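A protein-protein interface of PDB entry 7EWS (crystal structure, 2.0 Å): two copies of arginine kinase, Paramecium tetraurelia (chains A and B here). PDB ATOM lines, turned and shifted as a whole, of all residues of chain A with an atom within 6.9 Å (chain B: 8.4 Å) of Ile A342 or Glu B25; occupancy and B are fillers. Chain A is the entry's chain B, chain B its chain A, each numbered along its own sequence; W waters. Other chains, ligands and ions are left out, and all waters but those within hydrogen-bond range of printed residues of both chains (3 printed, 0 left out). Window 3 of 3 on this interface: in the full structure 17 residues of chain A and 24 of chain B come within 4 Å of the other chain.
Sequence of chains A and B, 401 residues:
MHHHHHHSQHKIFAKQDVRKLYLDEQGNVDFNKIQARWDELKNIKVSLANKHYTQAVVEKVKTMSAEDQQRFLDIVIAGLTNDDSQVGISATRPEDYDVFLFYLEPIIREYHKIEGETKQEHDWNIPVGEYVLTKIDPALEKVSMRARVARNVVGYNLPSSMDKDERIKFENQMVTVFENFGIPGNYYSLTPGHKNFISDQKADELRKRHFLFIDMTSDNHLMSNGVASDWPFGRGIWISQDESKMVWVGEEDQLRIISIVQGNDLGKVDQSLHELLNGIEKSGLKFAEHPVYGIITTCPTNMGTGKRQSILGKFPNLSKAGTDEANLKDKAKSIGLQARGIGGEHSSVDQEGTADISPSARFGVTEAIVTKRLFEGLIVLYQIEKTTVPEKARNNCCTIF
The backbone carbonyl oxygen of Val A349 is in hydrogen-bond range of the side-chain amino group of Lys B20.
O of Gly A341 lies close to OG of Ser A347, 3.3 Å away. The side-chain carboxylate (OD1) of Asp B24 lies within hydrogen-bond range of the backbone NH (N) of Asn B28 (3.0 Å). The side-chain hydroxyl of Ser A347 lies within hydrogen-bond range of the backbone NH of Gly A343. OD1 of Asp B24 is in hydrogen-bond range of N of Gln B26, 2.9 Å away. OG of Ser A347 is in hydrogen-bond range of O of Gly A344 (2.6 Å). The backbone carbonyl oxygen (O) of Leu B23 lies within hydrogen-bond range of the side-chain amino group (NZ) of Lys B33 (2.7 Å).
Ile A342 touches Glu B25 (CD1 to O, 3.98 Å). Ile A342 touches Gln B26 (O to O, 3.6 Å). CA of Gly B27 touches CG1 of Ile A342 (3.8 Å). Gly A343 touches Gly B27 (CA to O, 3.7 Å). Asn B28 touches Gly A343. Gln B70 touches Ser A347 (NE2 to CB, 3.7 Å). OG of Ser A348 touches CG of Lys B20 (3.98 Å). CD1 of Leu B23 touches CB of Ser A348, at 3.6 Å.
Printed residues of chain A within 4 Å of Glu B25: Ile A342. No residue of chain B comes within 4 Å of Gly A341. Printed residues of chain A within 4 Å of Lys B20: Ser A348 and Val A349. Of the printed residues of chain B, Ser A347 touches Gln B70 (3.7 Å). Printed residues of chain A within 4 Å of Gly B27: Ile A342 and Gly A343. The nearest printed residue of chain A that does not touch Glu B25 is Asp A350 (5.0 Å).
Printed residues of chain A that touch a printed residue of chain B: Ile A342, Gly A343, Ser A347, Ser A348 and Val A349.
No position is printed for both chains.
Water W2 lies within hydrogen-bond range of the backbone carbonyl oxygen (O) of Gly B27, the backbone NH (N) of Ser A348 and the backbone NH (N) of Gly A343. Water W1 lies within hydrogen-bond range of O of Gly A343 (2.6 Å), ND2 of Asn B28 (2.7 Å) and NE2 of Gln B70 (3.0 Å). Water W3 lies within hydrogen-bond range of OD2 of Asp A350 (2.7 Å) and O of Glu B25 (2.9 Å).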
ATOM      1  N   ARG A 146     -21.057  25.488  15.841  1.00  0.00           N
ATOM      2  CA  ARG A 146     -22.013  26.250  14.997  1.00  0.00           C
ATOM      3  C   ARG A 146     -23.243  26.595  15.830  1.00  0.00           C
ATOM      4  O   ARG A 146     -23.744  25.735  16.587  1.00  0.00           O
ATOM      5  CB  ARG A 146     -22.448  25.466  13.755  1.00  0.00           C
ATOM      6  CG  ARG A 146     -21.307  24.811  12.989  1.00  0.00           C
ATOM      7  CD  ARG A 146     -21.187  23.323  13.254  1.00  0.00           C
ATOM      8  NE  ARG A 146     -22.098  22.544  12.412  1.00  0.00           N
ATOM      9  CZ  ARG A 146     -21.834  22.109  11.170  1.00  0.00           C
ATOM     10  NH1 ARG A 146     -22.743  21.395  10.517  1.00  0.00           N
ATOM     11  NH2 ARG A 146     -20.671  22.376  10.590  1.00  0.00           N
ATOM     12  N   LEU A 312     -19.583  19.441  15.092  1.00  0.00           N
ATOM     13  CA  LEU A 312     -19.154  18.250  14.320  1.00  0.00           C
ATOM     14  C   LEU A 312     -18.199  17.450  15.206  1.00  0.00           C
ATOM     15  O   LEU A 312     -17.165  18.000  15.571  1.00  0.00           O
ATOM     16  CB  LEU A 312     -18.433  18.694  13.045  1.00  0.00           C
ATOM     17  CG  LEU A 312     -19.297  19.406  12.015  1.00  0.00           C
ATOM     18  CD1 LEU A 312     -18.529  19.547  10.714  1.00  0.00           C
ATOM     19  CD2 LEU A 312     -20.600  18.666  11.784  1.00  0.00           C
ATOM     20  N   GLY A 313     -18.554  16.216  15.553  1.00  0.00           N
ATOM     21  CA  GLY A 313     -17.668  15.291  16.285  1.00  0.00           C
ATOM     22  C   GLY A 313     -17.410  14.034  15.480  1.00  0.00           C
ATOM     23  O   GLY A 313     -18.185  13.773  14.523  1.00  0.00           O
ATOM     24  N   ARG A 340     -26.771  13.623  13.202  1.00  0.00           N
ATOM     25  CA  ARG A 340     -27.144  13.657  11.768  1.00  0.00           C
ATOM     26  C   ARG A 340     -25.857  13.627  10.950  1.00  0.00           C
ATOM     27  O   ARG A 340     -24.760  13.864  11.535  1.00  0.00           O
ATOM     28  CB  ARG A 340     -27.938  14.928  11.433  1.00  0.00           C
ATOM     29  CG  ARG A 340     -29.269  15.071  12.167  1.00  0.00           C
ATOM     30  CD  ARG A 340     -29.879  16.403  11.783  1.00  0.00           C
ATOM     31  NE  ARG A 340     -31.275  16.668  12.120  1.00  0.00           N
ATOM     32  CZ  ARG A 340     -32.172  15.799  12.600  1.00  0.00           C
ATOM     33  NH1 ARG A 340     -31.851  14.545  12.856  1.00  0.00           N
ATOM     34  NH2 ARG A 340     -33.404  16.213  12.837  1.00  0.00           N
ATOM     35  N   GLY A 341     -25.992  13.413   9.640  1.00  0.00           N
ATOM     36  CA  GLY A 341     -24.845  13.480   8.723  1.00  0.00           C
ATOM     37  C   GLY A 341     -24.271  14.889   8.684  1.00  0.00           C
ATOM     38  O   GLY A 341     -24.911  15.818   9.199  1.00  0.00           O
ATOM     39  N   ILE A 342     -23.105  15.068   8.079  1.00  0.00           N
ATOM     40  CA  ILE A 342     -22.438  16.403   8.021  1.00  0.00           C
ATOM     41  C   ILE A 342     -23.069  17.300   6.947  1.00  0.00           C
ATOM     42  O   ILE A 342     -22.773  18.489   6.960  1.00  0.00           O
ATOM     43  CB  ILE A 342     -20.926  16.233   7.833  1.00  0.00           C
ATOM     44  CG1 ILE A 342     -20.614  15.351   6.627  1.00  0.00           C
ATOM     45  CG2 ILE A 342     -20.343  15.688   9.116  1.00  0.00           C
ATOM     46  CD1 ILE A 342     -19.152  15.072   6.424  1.00  0.00           C
ATOM     47  N   GLY A 343     -23.940  16.799   6.074  1.00  0.00           N
ATOM     48  CA  GLY A 343     -24.527  17.626   4.998  1.00  0.00           C
ATOM     49  C   GLY A 343     -25.973  18.018   5.266  1.00  0.00           C
ATOM     50  O   GLY A 343     -26.725  18.218   4.283  1.00  0.00           O
ATOM     51  N   GLY A 344     -26.383  18.072   6.534  1.00  0.00           N
ATOM     52  CA  GLY A 344     -27.732  18.527   6.933  1.00  0.00           C
ATOM     53  C   GLY A 344     -28.682  17.352   7.099  1.00  0.00           C
ATOM     54  O   GLY A 344     -28.210  16.189   7.243  1.00  0.00           O
ATOM     55  N   SER A 347     -28.645  13.423   5.222  1.00  0.00           N
ATOM     56  CA  SER A 347     -27.250  13.329   4.717  1.00  0.00           C
ATOM     57  C   SER A 347     -26.532  12.135   5.369  1.00  0.00           C
ATOM     58  O   SER A 347     -27.194  11.307   5.959  1.00  0.00           O
ATOM     59  CB  SER A 347     -26.516  14.629   4.905  1.00  0.00           C
ATOM     60  OG  SER A 347     -26.200  14.850   6.278  1.00  0.00           O
ATOM     61  N   SER A 348     -25.221  12.010   5.223  1.00  0.00           N
ATOM     62  CA  SER A 348     -24.464  10.803   5.662  1.00  0.00           C
ATOM     63  C   SER A 348     -23.414  11.144   6.728  1.00  0.00           C
ATOM     64  O   SER A 348     -22.735  12.187   6.656  1.00  0.00           O
ATOM     65  CB  SER A 348     -23.818  10.090   4.493  1.00  0.00           C
ATOM     66  OG  SER A 348     -24.796   9.505   3.649  1.00  0.00           O
ATOM     67  N   VAL A 349     -23.246  10.231   7.677  1.00  0.00           N
ATOM     68  CA  VAL A 349     -22.068  10.239   8.589  1.00  0.00           C
ATOM     69  C   VAL A 349     -20.898   9.794   7.730  1.00  0.00           C
ATOM     70  O   VAL A 349     -21.119   8.856   6.939  1.00  0.00           O
ATOM     71  CB  VAL A 349     -22.307   9.285   9.763  1.00  0.00           C
ATOM     72  CG1 VAL A 349     -21.046   9.042  10.570  1.00  0.00           C
ATOM     73  CG2 VAL A 349     -23.443   9.789  10.625  1.00  0.00           C
ATOM     74  N   ASP A 350     -19.731  10.426   7.819  1.00  0.00           N
ATOM     75  CA  ASP A 350     -18.620  10.016   6.928  1.00  0.00           C
ATOM     76  C   ASP A 350     -17.838   8.863   7.545  1.00  0.00           C
ATOM     77  O   ASP A 350     -18.195   8.344   8.631  1.00  0.00           O
ATOM     78  CB  ASP A 350     -17.708  11.179   6.543  1.00  0.00           C
ATOM     79  CG  ASP A 350     -16.752  11.697   7.607  1.00  0.00           C
ATOM     80  OD1 ASP A 350     -16.413  10.951   8.570  1.00  0.00           O
ATOM     81  OD2 ASP A 350     -16.331  12.854   7.445  1.00  0.00           O
ATOM     82  N   GLY A 353     -16.567   8.712  11.024  1.00  0.00           N
ATOM     83  CA  GLY A 353     -17.648   8.810  12.014  1.00  0.00           C
ATOM     84  C   GLY A 353     -18.061  10.252  12.252  1.00  0.00           C
ATOM     85  O   GLY A 353     -18.696  10.518  13.274  1.00  0.00           O
ATOM     86  N   THR A 354     -17.717  11.157  11.342  1.00  0.00           N
ATOM     87  CA  THR A 354     -18.060  12.589  11.491  1.00  0.00           C
ATOM     88  C   THR A 354     -19.585  12.764  11.393  1.00  0.00           C
ATOM     89  O   THR A 354     -20.203  12.339  10.376  1.00  0.00           O
ATOM     90  CB  THR A 354     -17.295  13.503  10.530  1.00  0.00           C
ATOM     91  OG1 THR A 354     -15.952  13.038  10.455  1.00  0.00           O
ATOM     92  CG2 THR A 354     -17.295  14.942  11.001  1.00  0.00           C
ATOM     93  N   ALA A 355     -20.169  13.354  12.435  1.00  0.00           N
ATOM     94  CA  ALA A 355     -21.617  13.633  12.535  1.00  0.00           C
ATOM     95  C   ALA A 355     -21.853  15.015  13.162  1.00  0.00           C
ATOM     96  O   ALA A 355     -21.040  15.484  13.996  1.00  0.00           O
ATOM     97  CB  ALA A 355     -22.284  12.556  13.342  1.00  0.00           C
ATOM     98  N   ASP A 356     -22.958  15.630  12.779  1.00  0.00           N
ATOM     99  CA  ASP A 356     -23.466  16.857  13.423  1.00  0.00           C
ATOM    100  C   ASP A 356     -24.199  16.406  14.683  1.00  0.00           C
ATOM    101  O   ASP A 356     -25.101  15.553  14.560  1.00  0.00           O
ATOM    102  CB  ASP A 356     -24.345  17.654  12.462  1.00  0.00           C
ATOM    103  CG  ASP A 356     -24.965  18.876  13.108  1.00  0.00           C
ATOM    104  OD1 ASP A 356     -26.049  18.752  13.726  1.00  0.00           O
ATOM    105  OD2 ASP A 356     -24.350  19.938  13.007  1.00  0.00           O
ATOM    106  N   LYS B  20     -22.611   7.323  -0.354  1.00  0.00           N
ATOM    107  CA  LYS B  20     -21.408   8.095   0.059  1.00  0.00           C
ATOM    108  C   LYS B  20     -20.418   8.231  -1.103  1.00  0.00           C
ATOM    109  O   LYS B  20     -19.610   9.192  -1.074  1.00  0.00           O
ATOM    110  CB  LYS B  20     -20.735   7.449   1.272  1.00  0.00           C
ATOM    111  CG  LYS B  20     -21.589   7.425   2.529  1.00  0.00           C
ATOM    112  CD  LYS B  20     -20.896   6.753   3.687  1.00  0.00           C
ATOM    113  CE  LYS B  20     -21.818   6.494   4.852  1.00  0.00           C
ATOM    114  NZ  LYS B  20     -21.061   6.045   6.048  1.00  0.00           N
ATOM    115  N   TYR B  22     -21.081   9.353  -3.888  1.00  0.00           N
ATOM    116  CA  TYR B  22     -21.526  10.529  -4.682  1.00  0.00           C
ATOM    117  C   TYR B  22     -21.549  11.812  -3.830  1.00  0.00           C
ATOM    118  O   TYR B  22     -22.072  12.848  -4.294  1.00  0.00           O
ATOM    119  CB  TYR B  22     -22.869  10.195  -5.340  1.00  0.00           C
ATOM    120  CG  TYR B  22     -22.811   8.909  -6.118  1.00  0.00           C
ATOM    121  CD1 TYR B  22     -22.248   8.860  -7.385  1.00  0.00           C
ATOM    122  CD2 TYR B  22     -23.170   7.712  -5.525  1.00  0.00           C
ATOM    123  CE1 TYR B  22     -22.103   7.660  -8.064  1.00  0.00           C
ATOM    124  CE2 TYR B  22     -23.033   6.502  -6.186  1.00  0.00           C
ATOM    125  CZ  TYR B  22     -22.494   6.473  -7.464  1.00  0.00           C
ATOM    126  OH  TYR B  22     -22.385   5.281  -8.142  1.00  0.00           O
ATOM    127  N   LEU B  23     -20.929  11.771  -2.652  1.00  0.00           N
ATOM    128  CA  LEU B  23     -20.779  12.920  -1.733  1.00  0.00           C
ATOM    129  C   LEU B  23     -19.357  13.479  -1.824  1.00  0.00           C
ATOM    130  O   LEU B  23     -18.415  12.707  -2.056  1.00  0.00           O
ATOM    131  CB  LEU B  23     -21.099  12.463  -0.305  1.00  0.00           C
ATOM    132  CG  LEU B  23     -22.503  11.902  -0.103  1.00  0.00           C
ATOM    133  CD1 LEU B  23     -22.775  11.648   1.376  1.00  0.00           C
ATOM    134  CD2 LEU B  23     -23.548  12.836  -0.683  1.00  0.00           C
ATOM    135  N   ASP B  24     -19.221  14.776  -1.584  1.00  0.00           N
ATOM    136  CA  ASP B  24     -17.913  15.458  -1.464  1.00  0.00           C
ATOM    137  C   ASP B  24     -17.430  15.381  -0.006  1.00  0.00           C
ATOM    138  O   ASP B  24     -18.113  14.771   0.859  1.00  0.00           O
ATOM    139  CB  ASP B  24     -17.998  16.882  -2.038  1.00  0.00           C
ATOM    140  CG  ASP B  24     -18.808  17.890  -1.230  1.00  0.00           C
ATOM    141  OD1 ASP B  24     -19.057  17.647  -0.058  1.00  0.00           O
ATOM    142  OD2 ASP B  24     -19.174  18.922  -1.796  1.00  0.00           O
ATOM    143  N   GLU B  25     -16.286  16.007   0.264  1.00  0.00           N
ATOM    144  CA  GLU B  25     -15.609  15.996   1.594  1.00  0.00           C
ATOM    145  C   GLU B  25     -16.493  16.686   2.651  1.00  0.00           C
ATOM    146  O   GLU B  25     -16.400  16.296   3.815  1.00  0.00           O
ATOM    147  CB  GLU B  25     -14.244  16.681   1.502  1.00  0.00           C
ATOM    148  CG  GLU B  25     -13.511  16.450   0.179  1.00  0.00           C
ATOM    149  CD  GLU B  25     -14.154  17.083  -1.060  1.00  0.00           C
ATOM    150  OE1 GLU B  25     -14.442  16.328  -2.023  1.00  0.00           O
ATOM    151  OE2 GLU B  25     -14.396  18.330  -1.055  1.00  0.00           O
ATOM    152  N   GLN B  26     -17.360  17.629   2.287  1.00  0.00           N
ATOM    153  CA  GLN B  26     -18.252  18.335   3.257  1.00  0.00           C
ATOM    154  C   GLN B  26     -19.580  17.588   3.433  1.00  0.00           C
ATOM    155  O   GLN B  26     -20.448  18.103   4.174  1.00  0.00           O
ATOM    156  CB  GLN B  26     -18.632  19.746   2.818  1.00  0.00           C
ATOM    157  CG  GLN B  26     -17.771  20.341   1.726  1.00  0.00           C
ATOM    158  CD  GLN B  26     -16.550  20.963   2.332  1.00  0.00           C
ATOM    159  OE1 GLN B  26     -15.614  20.271   2.722  1.00  0.00           O
ATOM    160  NE2 GLN B  26     -16.581  22.278   2.437  1.00  0.00           N
ATOM    161  N   GLY B  27     -19.769  16.449   2.775  1.00  0.00           N
ATOM    162  CA  GLY B  27     -20.996  15.642   2.904  1.00  0.00           C
ATOM    163  C   GLY B  27     -22.105  16.133   1.975  1.00  0.00           C
ATOM    164  O   GLY B  27     -23.229  15.629   2.108  1.00  0.00           O
ATOM    165  N   ASN B  28     -21.811  17.072   1.065  1.00  0.00           N
ATOM    166  CA  ASN B  28     -22.797  17.561   0.063  1.00  0.00           C
ATOM    167  C   ASN B  28     -22.759  16.684  -1.195  1.00  0.00           C
ATOM    168  O   ASN B  28     -21.721  16.017  -1.455  1.00  0.00           O
ATOM    169  CB  ASN B  28     -22.570  19.020  -0.313  1.00  0.00           C
ATOM    170  CG  ASN B  28     -22.591  19.931   0.888  1.00  0.00           C
ATOM    171  OD1 ASN B  28     -21.702  20.779   1.025  1.00  0.00           O
ATOM    172  ND2 ASN B  28     -23.590  19.752   1.742  1.00  0.00           N
ATOM    173  N   VAL B  29     -23.854  16.705  -1.954  1.00  0.00           N
ATOM    174  CA  VAL B  29     -23.983  15.909  -3.208  1.00  0.00           C
ATOM    175  C   VAL B  29     -22.960  16.444  -4.228  1.00  0.00           C
ATOM    176  O   VAL B  29     -22.914  17.664  -4.442  1.00  0.00           O
ATOM    177  CB  VAL B  29     -25.419  15.906  -3.762  1.00  0.00           C
ATOM    178  CG1 VAL B  29     -25.463  15.193  -5.103  1.00  0.00           C
ATOM    179  CG2 VAL B  29     -26.402  15.266  -2.786  1.00  0.00           C
ATOM    180  N   ASP B  30     -22.133  15.546  -4.757  1.00  0.00           N
ATOM    181  CA  ASP B  30     -21.143  15.818  -5.823  1.00  0.00           C
ATOM    182  C   ASP B  30     -21.692  15.392  -7.189  1.00  0.00           C
ATOM    183  O   ASP B  30     -21.579  14.199  -7.579  1.00  0.00           O
ATOM    184  CB  ASP B  30     -19.835  15.077  -5.559  1.00  0.00           C
ATOM    185  CG  ASP B  30     -18.731  15.678  -6.393  1.00  0.00           C
ATOM    186  OD1 ASP B  30     -19.044  16.175  -7.480  1.00  0.00           O
ATOM    187  OD2 ASP B  30     -17.586  15.654  -5.939  1.00  0.00           O
ATOM    188  N   LYS B  33     -19.312  13.515  -9.561  1.00  0.00           N
ATOM    189  CA  LYS B  33     -19.275  12.043  -9.350  1.00  0.00           C
ATOM    190  C   LYS B  33     -20.537  11.379  -9.933  1.00  0.00           C
ATOM    191  O   LYS B  33     -20.416  10.269 -10.495  1.00  0.00           O
ATOM    192  CB  LYS B  33     -19.107  11.709  -7.865  1.00  0.00           C
ATOM    193  CG  LYS B  33     -17.822  12.242  -7.241  1.00  0.00           C
ATOM    194  CD  LYS B  33     -17.572  11.719  -5.848  1.00  0.00           C
ATOM    195  CE  LYS B  33     -16.287  12.222  -5.211  1.00  0.00           C
ATOM    196  NZ  LYS B  33     -16.359  12.097  -3.734  1.00  0.00           N
ATOM    197  N   ALA B  66     -30.403  21.779   0.279  1.00  0.00           N
ATOM    198  CA  ALA B  66     -29.453  20.669   0.518  1.00  0.00           C
ATOM    199  C   ALA B  66     -30.247  19.369   0.732  1.00  0.00           C
ATOM    200  O   ALA B  66     -29.800  18.300   0.253  1.00  0.00           O
ATOM    201  CB  ALA B  66     -28.573  20.970   1.707  1.00  0.00           C
ATOM    202  N   GLN B  70     -29.954  15.796  -1.472  1.00  0.00           N
ATOM    203  CA  GLN B  70     -29.663  14.485  -0.843  1.00  0.00           C
ATOM    204  C   GLN B  70     -30.762  13.489  -1.228  1.00  0.00           C
ATOM    205  O   GLN B  70     -30.452  12.348  -1.546  1.00  0.00           O
ATOM    206  CB  GLN B  70     -29.551  14.650   0.682  1.00  0.00           C
ATOM    207  CG  GLN B  70     -28.359  15.498   1.130  1.00  0.00           C
ATOM    208  CD  GLN B  70     -27.048  14.744   1.120  1.00  0.00           C
ATOM    209  OE1 GLN B  70     -26.998  13.528   0.960  1.00  0.00           O
ATOM    210  NE2 GLN B  70     -25.959  15.474   1.298  1.00  0.00           N
HETATM  211  O   HOH W   1     -25.887  18.396   1.799  1.00  0.00           O
HETATM  212  O   HOH W   2     -23.403  14.077   4.154  1.00  0.00           O
HETATM  213  O   HOH W   3     -16.539  13.648   4.870  1.00  0.00           O
